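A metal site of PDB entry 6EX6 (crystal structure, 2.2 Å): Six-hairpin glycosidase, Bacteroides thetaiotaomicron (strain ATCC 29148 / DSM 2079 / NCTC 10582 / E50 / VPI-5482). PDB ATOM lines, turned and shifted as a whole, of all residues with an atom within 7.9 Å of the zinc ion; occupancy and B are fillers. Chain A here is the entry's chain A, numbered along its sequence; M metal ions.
The backbone carbonyl oxygen of Cys 383 lies within hydrogen-bond range of the side-chain sulfur of Cys 317, 3.5 Å away. The side-chain sulfur (SG) of Cys 381 sits close to the side-chain sulfur (SG) of Cys 383 (3.5 Å). O of Cys 383 sits at hydrogen-bond distance from NZ of Lys 74 (2.9 Å). O of Cys 383 sits at hydrogen-bond distance from OG of Ser 386 (3.4 Å). The side-chain sulfur (SG) of Cys 384 sits close to the backbone carbonyl oxygen (O) of Tyr 363 (3.7 Å). The side-chain sulfur of Cys 384 lies close to the backbone carbonyl oxygen of Phe 362 (3.6 Å). The side-chain sulfur (SG) of Cys 317 sits at hydrogen-bond distance from the side-chain amide nitrogen (ND2) of Asn 387 (2.8 Å).
Within 4 Å of the zinc ion: Glu 315, Cys 317, Cys 383 and Cys 384. The nearest printed residue that does not touch the zinc ion is Tyr 363 (4.3 Å).
The zinc ion is bound by the side-chain carboxylate of Glu 315 (2.0 Å), the side-chain sulfur of Cys 383 (2.4 Å) and the side-chain sulfur of Cys 384 (2.7 Å). The zinc ion has three donor atoms within binding distance. Slightly farther from the zinc ion lies SG of Cys 317 (3.0 Å).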
ATOM      1  N   LYS A  74      19.277 -14.064  -4.748  1.00  0.00           N
ATOM      2  CA  LYS A  74      18.645 -13.211  -3.769  1.00  0.00           C
ATOM      3  C   LYS A  74      17.148 -12.938  -3.972  1.00  0.00           C
ATOM      4  O   LYS A  74      16.367 -12.875  -3.036  1.00  0.00           O
ATOM      5  CB  LYS A  74      19.371 -11.884  -3.694  1.00  0.00           C
ATOM      6  CG  LYS A  74      20.790 -12.013  -3.167  1.00  0.00           C
ATOM      7  CD  LYS A  74      21.173 -10.653  -2.676  1.00  0.00           C
ATOM      8  CE  LYS A  74      22.119  -9.909  -3.510  1.00  0.00           C
ATOM      9  NZ  LYS A  74      22.005  -8.469  -3.016  1.00  0.00           N
ATOM     10  N   TYR A 143      31.392 -14.995  -2.231  1.00  0.00           N
ATOM     11  CA  TYR A 143      30.206 -14.169  -2.175  1.00  0.00           C
ATOM     12  C   TYR A 143      29.035 -14.792  -2.933  1.00  0.00           C
ATOM     13  O   TYR A 143      27.907 -14.834  -2.406  1.00  0.00           O
ATOM     14  CB  TYR A 143      30.545 -12.819  -2.778  1.00  0.00           C
ATOM     15  CG  TYR A 143      29.438 -11.832  -2.884  1.00  0.00           C
ATOM     16  CD1 TYR A 143      29.149 -10.955  -1.806  1.00  0.00           C
ATOM     17  CD2 TYR A 143      28.656 -11.743  -4.060  1.00  0.00           C
ATOM     18  CE1 TYR A 143      28.180  -9.988  -1.917  1.00  0.00           C
ATOM     19  CE2 TYR A 143      27.633 -10.789  -4.160  1.00  0.00           C
ATOM     20  CZ  TYR A 143      27.398  -9.917  -3.081  1.00  0.00           C
ATOM     21  OH  TYR A 143      26.419  -8.958  -3.182  1.00  0.00           O
ATOM     22  N   HIS A 247      34.791  -0.937   2.796  1.00  0.00           N
ATOM     23  CA  HIS A 247      33.505  -1.088   2.135  1.00  0.00           C
ATOM     24  C   HIS A 247      32.503  -1.439   3.208  1.00  0.00           C
ATOM     25  O   HIS A 247      32.715  -2.380   3.982  1.00  0.00           O
ATOM     26  CB  HIS A 247      33.619  -2.167   1.043  1.00  0.00           C
ATOM     27  CG  HIS A 247      32.405  -2.293   0.162  1.00  0.00           C
ATOM     28  ND1 HIS A 247      32.357  -1.842  -1.152  1.00  0.00           N
ATOM     29  CD2 HIS A 247      31.202  -2.870   0.399  1.00  0.00           C
ATOM     30  CE1 HIS A 247      31.173  -2.151  -1.670  1.00  0.00           C
ATOM     31  NE2 HIS A 247      30.458  -2.785  -0.744  1.00  0.00           N
ATOM     32  N   VAL A 249      29.352  -2.538   3.241  1.00  0.00           N
ATOM     33  CA  VAL A 249      28.603  -3.769   3.143  1.00  0.00           C
ATOM     34  C   VAL A 249      29.471  -4.941   3.538  1.00  0.00           C
ATOM     35  O   VAL A 249      29.075  -5.796   4.298  1.00  0.00           O
ATOM     36  CB  VAL A 249      28.050  -4.043   1.732  1.00  0.00           C
ATOM     37  CG1 VAL A 249      27.313  -5.360   1.722  1.00  0.00           C
ATOM     38  CG2 VAL A 249      27.222  -2.898   1.181  1.00  0.00           C
ATOM     39  N   TYR A 253      28.417  -7.269   6.770  1.00  0.00           N
ATOM     40  CA  TYR A 253      28.275  -8.715   6.497  1.00  0.00           C
ATOM     41  C   TYR A 253      29.309  -9.535   7.311  1.00  0.00           C
ATOM     42  O   TYR A 253      28.941 -10.535   7.925  1.00  0.00           O
ATOM     43  CB  TYR A 253      28.406  -9.001   4.992  1.00  0.00           C
ATOM     44  CG  TYR A 253      27.171  -8.687   4.158  1.00  0.00           C
ATOM     45  CD1 TYR A 253      26.044  -8.014   4.681  1.00  0.00           C
ATOM     46  CD2 TYR A 253      27.119  -9.084   2.843  1.00  0.00           C
ATOM     47  CE1 TYR A 253      24.927  -7.776   3.887  1.00  0.00           C
ATOM     48  CE2 TYR A 253      26.022  -8.827   2.028  1.00  0.00           C
ATOM     49  CZ  TYR A 253      24.908  -8.216   2.539  1.00  0.00           C
ATOM     50  OH  TYR A 253      23.857  -7.997   1.650  1.00  0.00           O
ATOM     51  N   GLU A 299      33.127   2.781  -1.760  1.00  0.00           N
ATOM     52  CA  GLU A 299      31.782   2.576  -1.186  1.00  0.00           C
ATOM     53  C   GLU A 299      31.871   2.359   0.352  1.00  0.00           C
ATOM     54  O   GLU A 299      31.243   1.469   0.866  1.00  0.00           O
ATOM     55  CB  GLU A 299      31.146   1.351  -1.853  1.00  0.00           C
ATOM     56  CG  GLU A 299      31.113   1.496  -3.363  1.00  0.00           C
ATOM     57  CD  GLU A 299      30.290   0.434  -4.041  1.00  0.00           C
ATOM     58  OE1 GLU A 299      30.765  -0.740  -4.076  1.00  0.00           O
ATOM     59  OE2 GLU A 299      29.174   0.765  -4.516  1.00  0.00           O
ATOM     60  N   TYR A 313      27.348   8.157   0.800  1.00  0.00           N
ATOM     61  CA  TYR A 313      27.109   6.941   0.015  1.00  0.00           C
ATOM     62  C   TYR A 313      25.887   6.179   0.555  1.00  0.00           C
ATOM     63  O   TYR A 313      24.872   6.098  -0.178  1.00  0.00           O
ATOM     64  CB  TYR A 313      28.331   6.069  -0.105  1.00  0.00           C
ATOM     65  CG  TYR A 313      28.313   5.247  -1.357  1.00  0.00           C
ATOM     66  CD1 TYR A 313      28.540   5.850  -2.605  1.00  0.00           C
ATOM     67  CD2 TYR A 313      28.100   3.888  -1.312  1.00  0.00           C
ATOM     68  CE1 TYR A 313      28.545   5.117  -3.748  1.00  0.00           C
ATOM     69  CE2 TYR A 313      28.100   3.118  -2.455  1.00  0.00           C
ATOM     70  CZ  TYR A 313      28.297   3.765  -3.683  1.00  0.00           C
ATOM     71  OH  TYR A 313      28.364   3.077  -4.831  1.00  0.00           O
ATOM     72  N   GLU A 315      24.711   3.320   0.980  1.00  0.00           N
ATOM     73  CA  GLU A 315      24.164   2.247   0.153  1.00  0.00           C
ATOM     74  C   GLU A 315      22.991   1.498   0.761  1.00  0.00           C
ATOM     75  O   GLU A 315      23.072   1.096   1.914  1.00  0.00           O
ATOM     76  CB  GLU A 315      25.291   1.259  -0.198  1.00  0.00           C
ATOM     77  CG  GLU A 315      24.827   0.174  -1.173  1.00  0.00           C
ATOM     78  CD  GLU A 315      25.931  -0.755  -1.694  1.00  0.00           C
ATOM     79  OE1 GLU A 315      27.171  -0.513  -1.578  1.00  0.00           O
ATOM     80  OE2 GLU A 315      25.504  -1.775  -2.255  1.00  0.00           O
ATOM     81  N   THR A 316      21.937   1.239  -0.023  1.00  0.00           N
ATOM     82  CA  THR A 316      20.819   0.509   0.485  1.00  0.00           C
ATOM     83  C   THR A 316      21.255  -0.815   1.050  1.00  0.00           C
ATOM     84  O   THR A 316      20.883  -1.142   2.196  1.00  0.00           O
ATOM     85  CB  THR A 316      19.749   0.276  -0.576  1.00  0.00           C
ATOM     86  OG1 THR A 316      19.362   1.548  -1.148  1.00  0.00           O
ATOM     87  CG2 THR A 316      18.600  -0.395   0.028  1.00  0.00           C
ATOM     88  N   CYS A 317      22.174  -1.499   0.382  1.00  0.00           N
ATOM     89  CA  CYS A 317      22.718  -2.786   0.865  1.00  0.00           C
ATOM     90  C   CYS A 317      23.358  -2.662   2.259  1.00  0.00           C
ATOM     91  O   CYS A 317      23.254  -3.565   3.100  1.00  0.00           O
ATOM     92  CB  CYS A 317      23.782  -3.338  -0.107  1.00  0.00           C
ATOM     93  SG  CYS A 317      23.292  -4.721  -1.176  1.00  0.00           S
ATOM     94  N   ALA A 318      24.023  -1.539   2.496  1.00  0.00           N
ATOM     95  CA  ALA A 318      24.709  -1.294   3.763  1.00  0.00           C
ATOM     96  C   ALA A 318      23.713  -1.089   4.908  1.00  0.00           C
ATOM     97  O   ALA A 318      23.964  -1.466   6.048  1.00  0.00           O
ATOM     98  CB  ALA A 318      25.674  -0.152   3.654  1.00  0.00           C
ATOM     99  N   ILE A 320      20.720  -2.346   5.034  1.00  0.00           N
ATOM    100  CA  ILE A 320      20.237  -3.677   5.277  1.00  0.00           C
ATOM    101  C   ILE A 320      21.239  -4.421   6.174  1.00  0.00           C
ATOM    102  O   ILE A 320      20.837  -4.984   7.182  1.00  0.00           O
ATOM    103  CB  ILE A 320      19.926  -4.440   3.953  1.00  0.00           C
ATOM    104  CG1 ILE A 320      18.672  -3.877   3.327  1.00  0.00           C
ATOM    105  CG2 ILE A 320      19.726  -5.923   4.214  1.00  0.00           C
ATOM    106  CD1 ILE A 320      18.416  -4.236   1.874  1.00  0.00           C
ATOM    107  N   PHE A 362      17.155   2.927  -4.940  1.00  0.00           N
ATOM    108  CA  PHE A 362      18.328   3.729  -4.812  1.00  0.00           C
ATOM    109  C   PHE A 362      19.480   2.791  -4.477  1.00  0.00           C
ATOM    110  O   PHE A 362      19.313   1.788  -3.803  1.00  0.00           O
ATOM    111  CB  PHE A 362      18.160   4.740  -3.708  1.00  0.00           C
ATOM    112  CG  PHE A 362      17.672   6.074  -4.153  1.00  0.00           C
ATOM    113  CD1 PHE A 362      18.062   6.611  -5.346  1.00  0.00           C
ATOM    114  CD2 PHE A 362      16.812   6.782  -3.359  1.00  0.00           C
ATOM    115  CE1 PHE A 362      17.613   7.838  -5.742  1.00  0.00           C
ATOM    116  CE2 PHE A 362      16.353   8.018  -3.757  1.00  0.00           C
ATOM    117  CZ  PHE A 362      16.764   8.526  -4.956  1.00  0.00           C
ATOM    118  N   TYR A 363      20.639   3.120  -4.999  1.00  0.00           N
ATOM    119  CA  TYR A 363      21.855   2.421  -4.710  1.00  0.00           C
ATOM    120  C   TYR A 363      22.371   3.318  -3.580  1.00  0.00           C
ATOM    121  O   TYR A 363      22.226   2.948  -2.469  1.00  0.00           O
ATOM    122  CB  TYR A 363      22.722   2.329  -5.967  1.00  0.00           C
ATOM    123  CG  TYR A 363      23.990   1.495  -5.970  1.00  0.00           C
ATOM    124  CD1 TYR A 363      24.832   1.444  -4.883  1.00  0.00           C
ATOM    125  CD2 TYR A 363      24.384   0.815  -7.116  1.00  0.00           C
ATOM    126  CE1 TYR A 363      25.992   0.706  -4.928  1.00  0.00           C
ATOM    127  CE2 TYR A 363      25.540   0.083  -7.169  1.00  0.00           C
ATOM    128  CZ  TYR A 363      26.352   0.042  -6.074  1.00  0.00           C
ATOM    129  OH  TYR A 363      27.473  -0.664  -6.119  1.00  0.00           O
ATOM    130  N   PRO A 364      22.889   4.504  -3.841  1.00  0.00           N
ATOM    131  CA  PRO A 364      23.287   5.411  -2.761  1.00  0.00           C
ATOM    132  C   PRO A 364      22.104   6.206  -2.216  1.00  0.00           C
ATOM    133  O   PRO A 364      21.190   6.482  -2.921  1.00  0.00           O
ATOM    134  CB  PRO A 364      24.252   6.346  -3.421  1.00  0.00           C
ATOM    135  CG  PRO A 364      24.768   5.630  -4.565  1.00  0.00           C
ATOM    136  CD  PRO A 364      23.693   4.732  -5.042  1.00  0.00           C
ATOM    137  N   PHE A 379      19.670  -1.695 -12.151  1.00  0.00           N
ATOM    138  CA  PHE A 379      20.994  -1.070 -12.389  1.00  0.00           C
ATOM    139  C   PHE A 379      21.854  -2.168 -12.961  1.00  0.00           C
ATOM    140  O   PHE A 379      21.515  -3.336 -12.853  1.00  0.00           O
ATOM    141  CB  PHE A 379      21.706  -0.594 -11.103  1.00  0.00           C
ATOM    142  CG  PHE A 379      20.952   0.424 -10.279  1.00  0.00           C
ATOM    143  CD1 PHE A 379      21.068   1.793 -10.552  1.00  0.00           C
ATOM    144  CD2 PHE A 379      20.218   0.030  -9.191  1.00  0.00           C
ATOM    145  CE1 PHE A 379      20.363   2.740  -9.828  1.00  0.00           C
ATOM    146  CE2 PHE A 379      19.514   0.976  -8.429  1.00  0.00           C
ATOM    147  CZ  PHE A 379      19.586   2.330  -8.748  1.00  0.00           C
ATOM    148  N   CYS A 381      24.739  -2.939 -11.718  1.00  0.00           N
ATOM    149  CA  CYS A 381      25.019  -3.629 -10.509  1.00  0.00           C
ATOM    150  C   CYS A 381      23.745  -3.524  -9.692  1.00  0.00           C
ATOM    151  O   CYS A 381      23.452  -2.484  -9.121  1.00  0.00           O
ATOM    152  CB  CYS A 381      26.243  -3.076  -9.759  1.00  0.00           C
ATOM    153  SG  CYS A 381      26.479  -3.756  -8.062  1.00  0.00           S
ATOM    154  N   ALA A 382      23.012  -4.643  -9.621  1.00  0.00           N
ATOM    155  CA  ALA A 382      21.713  -4.678  -9.018  1.00  0.00           C
ATOM    156  C   ALA A 382      21.699  -5.258  -7.591  1.00  0.00           C
ATOM    157  O   ALA A 382      20.653  -5.740  -7.138  1.00  0.00           O
ATOM    158  CB  ALA A 382      20.723  -5.437  -9.928  1.00  0.00           C
ATOM    159  N   CYS A 383      22.777  -5.062  -6.838  1.00  0.00           N
ATOM    160  CA  CYS A 383      22.854  -5.594  -5.452  1.00  0.00           C
ATOM    161  C   CYS A 383      21.764  -5.034  -4.516  1.00  0.00           C
ATOM    162  O   CYS A 383      21.161  -5.770  -3.713  1.00  0.00           O
ATOM    163  CB  CYS A 383      24.260  -5.290  -4.846  1.00  0.00           C
ATOM    164  SG  CYS A 383      24.774  -3.550  -5.045  1.00  0.00           S
ATOM    165  N   CYS A 384      21.539  -3.739  -4.664  1.00  0.00           N
ATOM    166  CA  CYS A 384      20.540  -3.047  -3.877  1.00  0.00           C
ATOM    167  C   CYS A 384      19.183  -3.717  -4.147  1.00  0.00           C
ATOM    168  O   CYS A 384      18.734  -4.513  -3.320  1.00  0.00           O
ATOM    169  CB  CYS A 384      20.549  -1.520  -4.146  1.00  0.00           C
ATOM    170  SG  CYS A 384      21.974  -0.571  -3.512  1.00  0.00           S
ATOM    171  N   PRO A 385      18.572  -3.485  -5.326  1.00  0.00           N
ATOM    172  CA  PRO A 385      17.243  -4.049  -5.580  1.00  0.00           C
ATOM    173  C   PRO A 385      17.095  -5.516  -5.196  1.00  0.00           C
ATOM    174  O   PRO A 385      16.083  -5.861  -4.602  1.00  0.00           O
ATOM    175  CB  PRO A 385      17.083  -3.951  -7.112  1.00  0.00           C
ATOM    176  CG  PRO A 385      17.953  -2.814  -7.489  1.00  0.00           C
ATOM    177  CD  PRO A 385      19.142  -2.903  -6.534  1.00  0.00           C
ATOM    178  N   SER A 386      18.073  -6.371  -5.491  1.00  0.00           N
ATOM    179  CA  SER A 386      17.893  -7.791  -5.124  1.00  0.00           C
ATOM    180  C   SER A 386      17.955  -7.978  -3.605  1.00  0.00           C
ATOM    181  O   SER A 386      17.310  -8.891  -3.062  1.00  0.00           O
ATOM    182  CB  SER A 386      18.860  -8.740  -5.852  1.00  0.00           C
ATOM    183  OG  SER A 386      20.204  -8.382  -5.667  1.00  0.00           O
ATOM    184  N   ASN A 387      18.661  -7.094  -2.920  1.00  0.00           N
ATOM    185  CA  ASN A 387      18.786  -7.118  -1.463  1.00  0.00           C
ATOM    186  C   ASN A 387      17.474  -6.711  -0.839  1.00  0.00           C
ATOM    187  O   ASN A 387      16.980  -7.359   0.025  1.00  0.00           O
ATOM    188  CB  ASN A 387      19.950  -6.251  -0.993  1.00  0.00           C
ATOM    189  CG  ASN A 387      20.676  -6.815   0.219  1.00  0.00           C
ATOM    190  OD1 ASN A 387      20.230  -7.739   0.843  1.00  0.00           O
ATOM    191  ND2 ASN A 387      21.760  -6.205   0.570  1.00  0.00           N
ATOM    192  N   VAL A 388      16.917  -5.606  -1.322  1.00  0.00           N
ATOM    193  CA  VAL A 388      15.589  -5.134  -0.932  1.00  0.00           C
ATOM    194  C   VAL A 388      14.535  -6.208  -1.115  1.00  0.00           C
ATOM    195  O   VAL A 388      13.695  -6.410  -0.248  1.00  0.00           O
ATOM    196  CB  VAL A 388      15.172  -3.865  -1.678  1.00  0.00           C
ATOM    197  CG1 VAL A 388      13.653  -3.614  -1.533  1.00  0.00           C
ATOM    198  CG2 VAL A 388      15.959  -2.702  -1.145  1.00  0.00           C
HETATM  199 ZN    ZN M   1      23.797  -2.500  -3.091  1.00  0.00          ZN
